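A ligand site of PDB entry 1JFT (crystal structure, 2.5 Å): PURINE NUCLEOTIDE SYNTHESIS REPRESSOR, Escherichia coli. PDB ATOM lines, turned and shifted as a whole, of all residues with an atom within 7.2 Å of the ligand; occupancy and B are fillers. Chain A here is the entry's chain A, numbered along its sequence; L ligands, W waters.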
ATOM      1  N   THR A  66      -2.097 -20.206 -13.923  1.00  0.00           N
ATOM      2  CA  THR A  66      -3.327 -19.452 -13.889  1.00  0.00           C
ATOM      3  C   THR A  66      -3.506 -18.788 -15.249  1.00  0.00           C
ATOM      4  O   THR A  66      -4.560 -18.892 -15.861  1.00  0.00           O
ATOM      5  CB  THR A  66      -3.292 -18.418 -12.833  1.00  0.00           C
ATOM      6  OG1 THR A  66      -3.285 -19.056 -11.548  1.00  0.00           O
ATOM      7  CG2 THR A  66      -4.526 -17.605 -12.919  1.00  0.00           C
ATOM      8  N   ALA A  70       0.246 -12.262 -18.173  1.00  0.00           N
ATOM      9  CA  ALA A  70       0.655 -11.383 -17.090  1.00  0.00           C
ATOM     10  C   ALA A  70       2.164 -11.424 -16.869  1.00  0.00           C
ATOM     11  O   ALA A  70       2.754 -12.490 -16.674  1.00  0.00           O
ATOM     12  CB  ALA A  70      -0.085 -11.789 -15.813  1.00  0.00           C
ATOM     13  N   ALA A  71       2.770 -10.252 -16.966  1.00  0.00           N
ATOM     14  CA  ALA A  71       4.216 -10.088 -16.819  1.00  0.00           C
ATOM     15  C   ALA A  71       4.811 -10.952 -15.742  1.00  0.00           C
ATOM     16  O   ALA A  71       5.736 -11.667 -15.986  1.00  0.00           O
ATOM     17  CB  ALA A  71       4.533  -8.616 -16.501  1.00  0.00           C
ATOM     18  N   TYR A  72       4.233 -10.863 -14.554  1.00  0.00           N
ATOM     19  CA  TYR A  72       4.663 -11.613 -13.410  1.00  0.00           C
ATOM     20  C   TYR A  72       4.764 -13.127 -13.850  1.00  0.00           C
ATOM     21  O   TYR A  72       5.873 -13.689 -14.000  1.00  0.00           O
ATOM     22  CB  TYR A  72       3.646 -11.372 -12.282  1.00  0.00           C
ATOM     23  CG  TYR A  72       3.970 -12.101 -10.987  1.00  0.00           C
ATOM     24  CD1 TYR A  72       3.131 -13.068 -10.464  1.00  0.00           C
ATOM     25  CD2 TYR A  72       5.122 -11.808 -10.301  1.00  0.00           C
ATOM     26  CE1 TYR A  72       3.437 -13.718  -9.286  1.00  0.00           C
ATOM     27  CE2 TYR A  72       5.436 -12.449  -9.115  1.00  0.00           C
ATOM     28  CZ  TYR A  72       4.596 -13.403  -8.618  1.00  0.00           C
ATOM     29  OH  TYR A  72       4.960 -14.014  -7.437  1.00  0.00           O
ATOM     30  N   PHE A  73       3.624 -13.729 -14.097  1.00  0.00           N
ATOM     31  CA  PHE A  73       3.573 -15.119 -14.527  1.00  0.00           C
ATOM     32  C   PHE A  73       4.497 -15.397 -15.665  1.00  0.00           C
ATOM     33  O   PHE A  73       5.280 -16.332 -15.629  1.00  0.00           O
ATOM     34  CB  PHE A  73       2.170 -15.450 -14.916  1.00  0.00           C
ATOM     35  CG  PHE A  73       1.229 -15.421 -13.744  1.00  0.00           C
ATOM     36  CD1 PHE A  73      -0.078 -14.971 -13.890  1.00  0.00           C
ATOM     37  CD2 PHE A  73       1.670 -15.822 -12.491  1.00  0.00           C
ATOM     38  CE1 PHE A  73      -0.938 -14.931 -12.805  1.00  0.00           C
ATOM     39  CE2 PHE A  73       0.810 -15.791 -11.408  1.00  0.00           C
ATOM     40  CZ  PHE A  73      -0.504 -15.331 -11.559  1.00  0.00           C
ATOM     41  N   SER A 123      -2.761 -19.698  -8.037  1.00  0.00           N
ATOM     42  CA  SER A 123      -3.190 -18.465  -7.347  1.00  0.00           C
ATOM     43  C   SER A 123      -4.088 -18.736  -6.201  1.00  0.00           C
ATOM     44  O   SER A 123      -3.693 -18.598  -5.101  1.00  0.00           O
ATOM     45  CB  SER A 123      -3.915 -17.550  -8.333  1.00  0.00           C
ATOM     46  OG  SER A 123      -3.061 -17.187  -9.413  1.00  0.00           O
ATOM     47  N   ASP A 145       3.022 -21.079  -5.402  1.00  0.00           N
ATOM     48  CA  ASP A 145       2.506 -19.798  -4.952  1.00  0.00           C
ATOM     49  C   ASP A 145       1.507 -19.698  -3.838  1.00  0.00           C
ATOM     50  O   ASP A 145       0.614 -18.858  -3.891  1.00  0.00           O
ATOM     51  CB  ASP A 145       1.880 -19.135  -6.165  1.00  0.00           C
ATOM     52  CG  ASP A 145       0.702 -19.942  -6.721  1.00  0.00           C
ATOM     53  OD1 ASP A 145       0.263 -19.692  -7.840  1.00  0.00           O
ATOM     54  OD2 ASP A 145       0.191 -20.816  -6.003  1.00  0.00           O
ATOM     55  N   ASP A 159       7.062 -17.583  -0.601  1.00  0.00           N
ATOM     56  CA  ASP A 159       7.649 -16.311  -1.018  1.00  0.00           C
ATOM     57  C   ASP A 159       7.819 -15.278   0.026  1.00  0.00           C
ATOM     58  O   ASP A 159       8.407 -14.295  -0.221  1.00  0.00           O
ATOM     59  CB  ASP A 159       7.054 -15.769  -2.302  1.00  0.00           C
ATOM     60  CG  ASP A 159       5.669 -15.255  -2.127  1.00  0.00           C
ATOM     61  OD1 ASP A 159       5.120 -14.716  -3.133  1.00  0.00           O
ATOM     62  OD2 ASP A 159       5.141 -15.382  -0.988  1.00  0.00           O
ATOM     63  N   PRO A 186      -6.155  -9.466  -5.141  1.00  0.00           N
ATOM     64  CA  PRO A 186      -7.170 -10.390  -4.611  1.00  0.00           C
ATOM     65  C   PRO A 186      -6.820 -10.933  -3.282  1.00  0.00           C
ATOM     66  O   PRO A 186      -5.733 -11.526  -3.085  1.00  0.00           O
ATOM     67  CB  PRO A 186      -7.162 -11.493  -5.622  1.00  0.00           C
ATOM     68  CG  PRO A 186      -6.785 -10.825  -6.903  1.00  0.00           C
ATOM     69  CD  PRO A 186      -5.858  -9.726  -6.559  1.00  0.00           C
ATOM     70  N   ARG A 189      -5.667 -14.530  -2.691  1.00  0.00           N
ATOM     71  CA  ARG A 189      -4.340 -15.011  -3.080  1.00  0.00           C
ATOM     72  C   ARG A 189      -3.244 -14.672  -2.084  1.00  0.00           C
ATOM     73  O   ARG A 189      -3.356 -13.735  -1.301  1.00  0.00           O
ATOM     74  CB  ARG A 189      -3.949 -14.492  -4.448  1.00  0.00           C
ATOM     75  CG  ARG A 189      -4.692 -15.133  -5.511  1.00  0.00           C
ATOM     76  CD  ARG A 189      -5.296 -14.120  -6.358  1.00  0.00           C
ATOM     77  NE  ARG A 189      -4.508 -13.951  -7.551  1.00  0.00           N
ATOM     78  CZ  ARG A 189      -5.014 -14.111  -8.757  1.00  0.00           C
ATOM     79  NH1 ARG A 189      -6.280 -14.462  -8.897  1.00  0.00           N
ATOM     80  NH2 ARG A 189      -4.263 -13.940  -9.820  1.00  0.00           N
ATOM     81  N   ASN A 190      -2.164 -15.450  -2.137  1.00  0.00           N
ATOM     82  CA  ASN A 190      -1.046 -15.208  -1.242  1.00  0.00           C
ATOM     83  C   ASN A 190      -0.477 -13.801  -1.481  1.00  0.00           C
ATOM     84  O   ASN A 190      -0.430 -12.949  -0.559  1.00  0.00           O
ATOM     85  CB  ASN A 190       0.079 -16.211  -1.488  1.00  0.00           C
ATOM     86  CG  ASN A 190       1.261 -15.920  -0.595  1.00  0.00           C
ATOM     87  OD1 ASN A 190       1.054 -15.724   0.624  1.00  0.00           O
ATOM     88  ND2 ASN A 190       2.471 -15.782  -1.180  1.00  0.00           N
ATOM     89  N   THR A 191      -0.051 -13.574  -2.730  1.00  0.00           N
ATOM     90  CA  THR A 191       0.500 -12.300  -3.153  1.00  0.00           C
ATOM     91  C   THR A 191      -0.540 -11.189  -2.966  1.00  0.00           C
ATOM     92  O   THR A 191      -0.229 -10.035  -3.161  1.00  0.00           O
ATOM     93  CB  THR A 191       0.914 -12.340  -4.571  1.00  0.00           C
ATOM     94  OG1 THR A 191      -0.174 -12.859  -5.308  1.00  0.00           O
ATOM     95  CG2 THR A 191       2.114 -13.252  -4.762  1.00  0.00           C
ATOM     96  N   GLY A 192      -1.754 -11.543  -2.564  1.00  0.00           N
ATOM     97  CA  GLY A 192      -2.823 -10.560  -2.323  1.00  0.00           C
ATOM     98  C   GLY A 192      -2.823 -10.201  -0.809  1.00  0.00           C
ATOM     99  O   GLY A 192      -2.192  -9.253  -0.361  1.00  0.00           O
ATOM    100  N   ARG A 195       0.776  -9.800   1.101  1.00  0.00           N
ATOM    101  CA  ARG A 195       1.469  -8.542   1.028  1.00  0.00           C
ATOM    102  C   ARG A 195       0.787  -7.496   1.857  1.00  0.00           C
ATOM    103  O   ARG A 195       1.418  -6.769   2.565  1.00  0.00           O
ATOM    104  CB  ARG A 195       1.606  -8.123  -0.439  1.00  0.00           C
ATOM    105  CG  ARG A 195       2.451  -9.153  -1.264  1.00  0.00           C
ATOM    106  CD  ARG A 195       2.471  -8.876  -2.776  1.00  0.00           C
ATOM    107  NE  ARG A 195       3.301  -9.833  -3.483  1.00  0.00           N
ATOM    108  CZ  ARG A 195       3.516  -9.794  -4.788  1.00  0.00           C
ATOM    109  NH1 ARG A 195       2.959  -8.833  -5.501  1.00  0.00           N
ATOM    110  NH2 ARG A 195       4.295 -10.705  -5.386  1.00  0.00           N
ATOM    111  N   ASP A 219      -6.936  -6.219  -8.849  1.00  0.00           N
ATOM    112  CA  ASP A 219      -6.998  -7.596  -9.370  1.00  0.00           C
ATOM    113  C   ASP A 219      -5.747  -7.919 -10.126  1.00  0.00           C
ATOM    114  O   ASP A 219      -5.727  -8.863 -10.913  1.00  0.00           O
ATOM    115  CB  ASP A 219      -8.242  -7.796 -10.253  1.00  0.00           C
ATOM    116  CG  ASP A 219      -8.191  -7.012 -11.575  1.00  0.00           C
ATOM    117  OD1 ASP A 219      -9.238  -6.986 -12.246  1.00  0.00           O
ATOM    118  OD2 ASP A 219      -7.163  -6.432 -11.971  1.00  0.00           O
ATOM    119  N   PHE A 220      -4.697  -7.128  -9.911  1.00  0.00           N
ATOM    120  CA  PHE A 220      -3.384  -7.292 -10.588  1.00  0.00           C
ATOM    121  C   PHE A 220      -3.399  -6.824 -12.013  1.00  0.00           C
ATOM    122  O   PHE A 220      -2.374  -6.913 -12.675  1.00  0.00           O
ATOM    123  CB  PHE A 220      -2.857  -8.736 -10.555  1.00  0.00           C
ATOM    124  CG  PHE A 220      -2.385  -9.149  -9.234  1.00  0.00           C
ATOM    125  CD1 PHE A 220      -1.315  -8.493  -8.661  1.00  0.00           C
ATOM    126  CD2 PHE A 220      -3.040 -10.159  -8.530  1.00  0.00           C
ATOM    127  CE1 PHE A 220      -0.873  -8.853  -7.416  1.00  0.00           C
ATOM    128  CE2 PHE A 220      -2.598 -10.541  -7.274  1.00  0.00           C
ATOM    129  CZ  PHE A 220      -1.508  -9.882  -6.724  1.00  0.00           C
ATOM    130  N   GLU A 221      -4.536  -6.338 -12.503  1.00  0.00           N
ATOM    131  CA  GLU A 221      -4.641  -5.834 -13.883  1.00  0.00           C
ATOM    132  C   GLU A 221      -4.673  -4.294 -13.828  1.00  0.00           C
ATOM    133  O   GLU A 221      -5.391  -3.672 -13.004  1.00  0.00           O
ATOM    134  CB  GLU A 221      -5.837  -6.430 -14.635  1.00  0.00           C
ATOM    135  CG  GLU A 221      -5.880  -7.936 -14.632  1.00  0.00           C
ATOM    136  CD  GLU A 221      -5.373  -8.576 -15.915  1.00  0.00           C
ATOM    137  OE1 GLU A 221      -4.231  -8.268 -16.335  1.00  0.00           O
ATOM    138  OE2 GLU A 221      -6.114  -9.409 -16.506  1.00  0.00           O
ATOM    139  N   GLY A 245      -0.151  -3.080  -4.624  1.00  0.00           N
ATOM    140  CA  GLY A 245       0.070  -4.528  -4.587  1.00  0.00           C
ATOM    141  C   GLY A 245       0.825  -5.286  -5.655  1.00  0.00           C
ATOM    142  O   GLY A 245       1.282  -6.377  -5.408  1.00  0.00           O
ATOM    143  N   GLY A 246       0.921  -4.726  -6.840  1.00  0.00           N
ATOM    144  CA  GLY A 246       1.605  -5.343  -7.969  1.00  0.00           C
ATOM    145  C   GLY A 246       1.993  -4.268  -8.996  1.00  0.00           C
ATOM    146  O   GLY A 246       1.254  -3.323  -9.304  1.00  0.00           O
ATOM    147  N   ASP A 247       3.171  -4.411  -9.521  1.00  0.00           N
ATOM    148  CA  ASP A 247       3.665  -3.500 -10.484  1.00  0.00           C
ATOM    149  C   ASP A 247       2.737  -3.167 -11.664  1.00  0.00           C
ATOM    150  O   ASP A 247       2.470  -1.982 -11.968  1.00  0.00           O
ATOM    151  CB  ASP A 247       4.994  -3.996 -10.969  1.00  0.00           C
ATOM    152  CG  ASP A 247       6.082  -3.796  -9.929  1.00  0.00           C
ATOM    153  OD1 ASP A 247       7.303  -3.978 -10.269  1.00  0.00           O
ATOM    154  OD2 ASP A 247       5.727  -3.403  -8.782  1.00  0.00           O
ATOM    155  N   ILE A 248       2.251  -4.188 -12.329  1.00  0.00           N
ATOM    156  CA  ILE A 248       1.380  -3.957 -13.455  1.00  0.00           C
ATOM    157  C   ILE A 248       0.176  -3.124 -13.003  1.00  0.00           C
ATOM    158  O   ILE A 248      -0.298  -2.276 -13.722  1.00  0.00           O
ATOM    159  CB  ILE A 248       0.966  -5.271 -14.131  1.00  0.00           C
ATOM    160  CG1 ILE A 248       2.204  -5.979 -14.673  1.00  0.00           C
ATOM    161  CG2 ILE A 248       0.022  -5.000 -15.306  1.00  0.00           C
ATOM    162  CD1 ILE A 248       3.083  -5.031 -15.409  1.00  0.00           C
ATOM    163  N   TYR A 273       5.103  -3.616  -6.178  1.00  0.00           N
ATOM    164  CA  TYR A 273       5.563  -4.934  -5.765  1.00  0.00           C
ATOM    165  C   TYR A 273       5.601  -5.944  -6.928  1.00  0.00           C
ATOM    166  O   TYR A 273       4.578  -6.138  -7.619  1.00  0.00           O
ATOM    167  CB  TYR A 273       4.560  -5.492  -4.780  1.00  0.00           C
ATOM    168  CG  TYR A 273       5.161  -6.508  -3.840  1.00  0.00           C
ATOM    169  CD1 TYR A 273       5.008  -6.396  -2.472  1.00  0.00           C
ATOM    170  CD2 TYR A 273       5.884  -7.595  -4.334  1.00  0.00           C
ATOM    171  CE1 TYR A 273       5.557  -7.326  -1.625  1.00  0.00           C
ATOM    172  CE2 TYR A 273       6.440  -8.548  -3.469  1.00  0.00           C
ATOM    173  CZ  TYR A 273       6.286  -8.410  -2.139  1.00  0.00           C
ATOM    174  OH  TYR A 273       6.848  -9.346  -1.322  1.00  0.00           O
ATOM    175  N   ASP A 274       6.779  -6.556  -7.088  1.00  0.00           N
ATOM    176  CA  ASP A 274       7.128  -7.620  -8.079  1.00  0.00           C
ATOM    177  C   ASP A 274       8.448  -7.418  -8.773  1.00  0.00           C
ATOM    178  O   ASP A 274       9.227  -8.342  -9.014  1.00  0.00           O
ATOM    179  CB  ASP A 274       6.087  -7.868  -9.149  1.00  0.00           C
ATOM    180  CG  ASP A 274       4.881  -8.676  -8.687  1.00  0.00           C
ATOM    181  OD1 ASP A 274       3.984  -8.844  -9.572  1.00  0.00           O
ATOM    182  OD2 ASP A 274       4.775  -9.107  -7.482  1.00  0.00           O
ATOM    183  N   VAL A 276       8.829  -6.339 -11.974  1.00  0.00           N
ATOM    184  CA  VAL A 276       8.769  -7.057 -13.247  1.00  0.00           C
ATOM    185  C   VAL A 276       9.842  -6.418 -14.115  1.00  0.00           C
ATOM    186  O   VAL A 276      10.191  -5.306 -13.896  1.00  0.00           O
ATOM    187  CB  VAL A 276       7.369  -6.981 -13.925  1.00  0.00           C
ATOM    188  CG1 VAL A 276       6.335  -7.716 -13.101  1.00  0.00           C
ATOM    189  CG2 VAL A 276       6.928  -5.545 -14.113  1.00  0.00           C
ATOM    190  N   GLN A 291      10.478  -9.631  -6.295  1.00  0.00           N
ATOM    191  CA  GLN A 291      10.080 -11.036  -6.034  1.00  0.00           C
ATOM    192  C   GLN A 291      11.117 -11.736  -6.803  1.00  0.00           C
ATOM    193  O   GLN A 291      11.336 -11.434  -7.975  1.00  0.00           O
ATOM    194  CB  GLN A 291       8.777 -11.353  -6.740  1.00  0.00           C
ATOM    195  CG  GLN A 291       8.275 -12.810  -6.583  1.00  0.00           C
ATOM    196  CD  GLN A 291       7.840 -13.102  -5.171  1.00  0.00           C
ATOM    197  OE1 GLN A 291       6.665 -13.370  -4.872  1.00  0.00           O
ATOM    198  NE2 GLN A 291       8.792 -13.026  -4.288  1.00  0.00           N
HETATM  199  N1  LIG L   1      -1.120 -11.865 -10.760  1.00  0.00           N
HETATM  200  C1  LIG L   1      -0.283 -11.015 -11.437  1.00  0.00           C
HETATM  201  N2  LIG L   1       0.851 -10.530 -10.950  1.00  0.00           N
HETATM  202  C2  LIG L   1       1.024 -10.929  -9.672  1.00  0.00           C
HETATM  203  C3  LIG L   1       0.255 -11.774  -8.903  1.00  0.00           C
HETATM  204  C4  LIG L   1      -0.925 -12.329  -9.456  1.00  0.00           C
HETATM  205  O1  LIG L   1      -1.747 -13.112  -8.949  1.00  0.00           O
HETATM  206  N3  LIG L   1       0.815 -11.938  -7.633  1.00  0.00           N
HETATM  207  C5  LIG L   1       1.895 -11.221  -7.674  1.00  0.00           C
HETATM  208  N4  LIG L   1       2.091 -10.579  -8.880  1.00  0.00           N
HETATM  209  O   HOH W   1       1.606  -9.187 -13.289  1.00  0.00           O
HETATM  210  O   HOH W   2      -0.048 -15.621  -7.820  1.00  0.00           O
HETATM  211  O   HOH W   3      -3.501 -12.443 -11.899  1.00  0.00           O
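Merely in contact with the ligand: Tyr 72 (3.1 Å), Phe 73 (3.6 Å), Arg 195 (3.4 Å) and Phe 220 (3.2 Å). The nearest printed residue that does not touch the ligand is Ser 123 (4.3 Å).
Water W3 bridges NH2 of Arg 189 (2.7 Å) and N1 of the ligand (2.7 Å). Water W1 bridges N2 of the ligand (2.8 Å) and N of Tyr 72 (3.4 Å).
The side-chain hydroxyl (OG1) of Thr 191 is in hydrogen-bond range of a nitrogen (N3) of the ligand (2.7 Å). OD1 of Asp 274 sits at hydrogen-bond distance from N4 of the ligand (2.7 Å). An oxygen (O1) of the ligand lies within hydrogen-bond range of the guanidinium group of Arg 189, 2.8 Å away.
The guanidinium group of Arg 195 lies within hydrogen-bond range of the backbone carbonyl oxygen of Gly 245 (3.0 Å). The side-chain carboxylate of Asp 274 is in salt-bridge range of the guanidinium group of Arg 195, 2.7 Å away. NH2 of Arg 189 sits at hydrogen-bond distance from OG of Ser 123, at 3.5 Å. The side-chain hydroxyl of Tyr 72 lies within hydrogen-bond range of the side-chain amide oxygen of Gln 291, 3.1 Å away. O of Asp 274 lies within hydrogen-bond range of N of Gln 291, at 3.3 Å.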
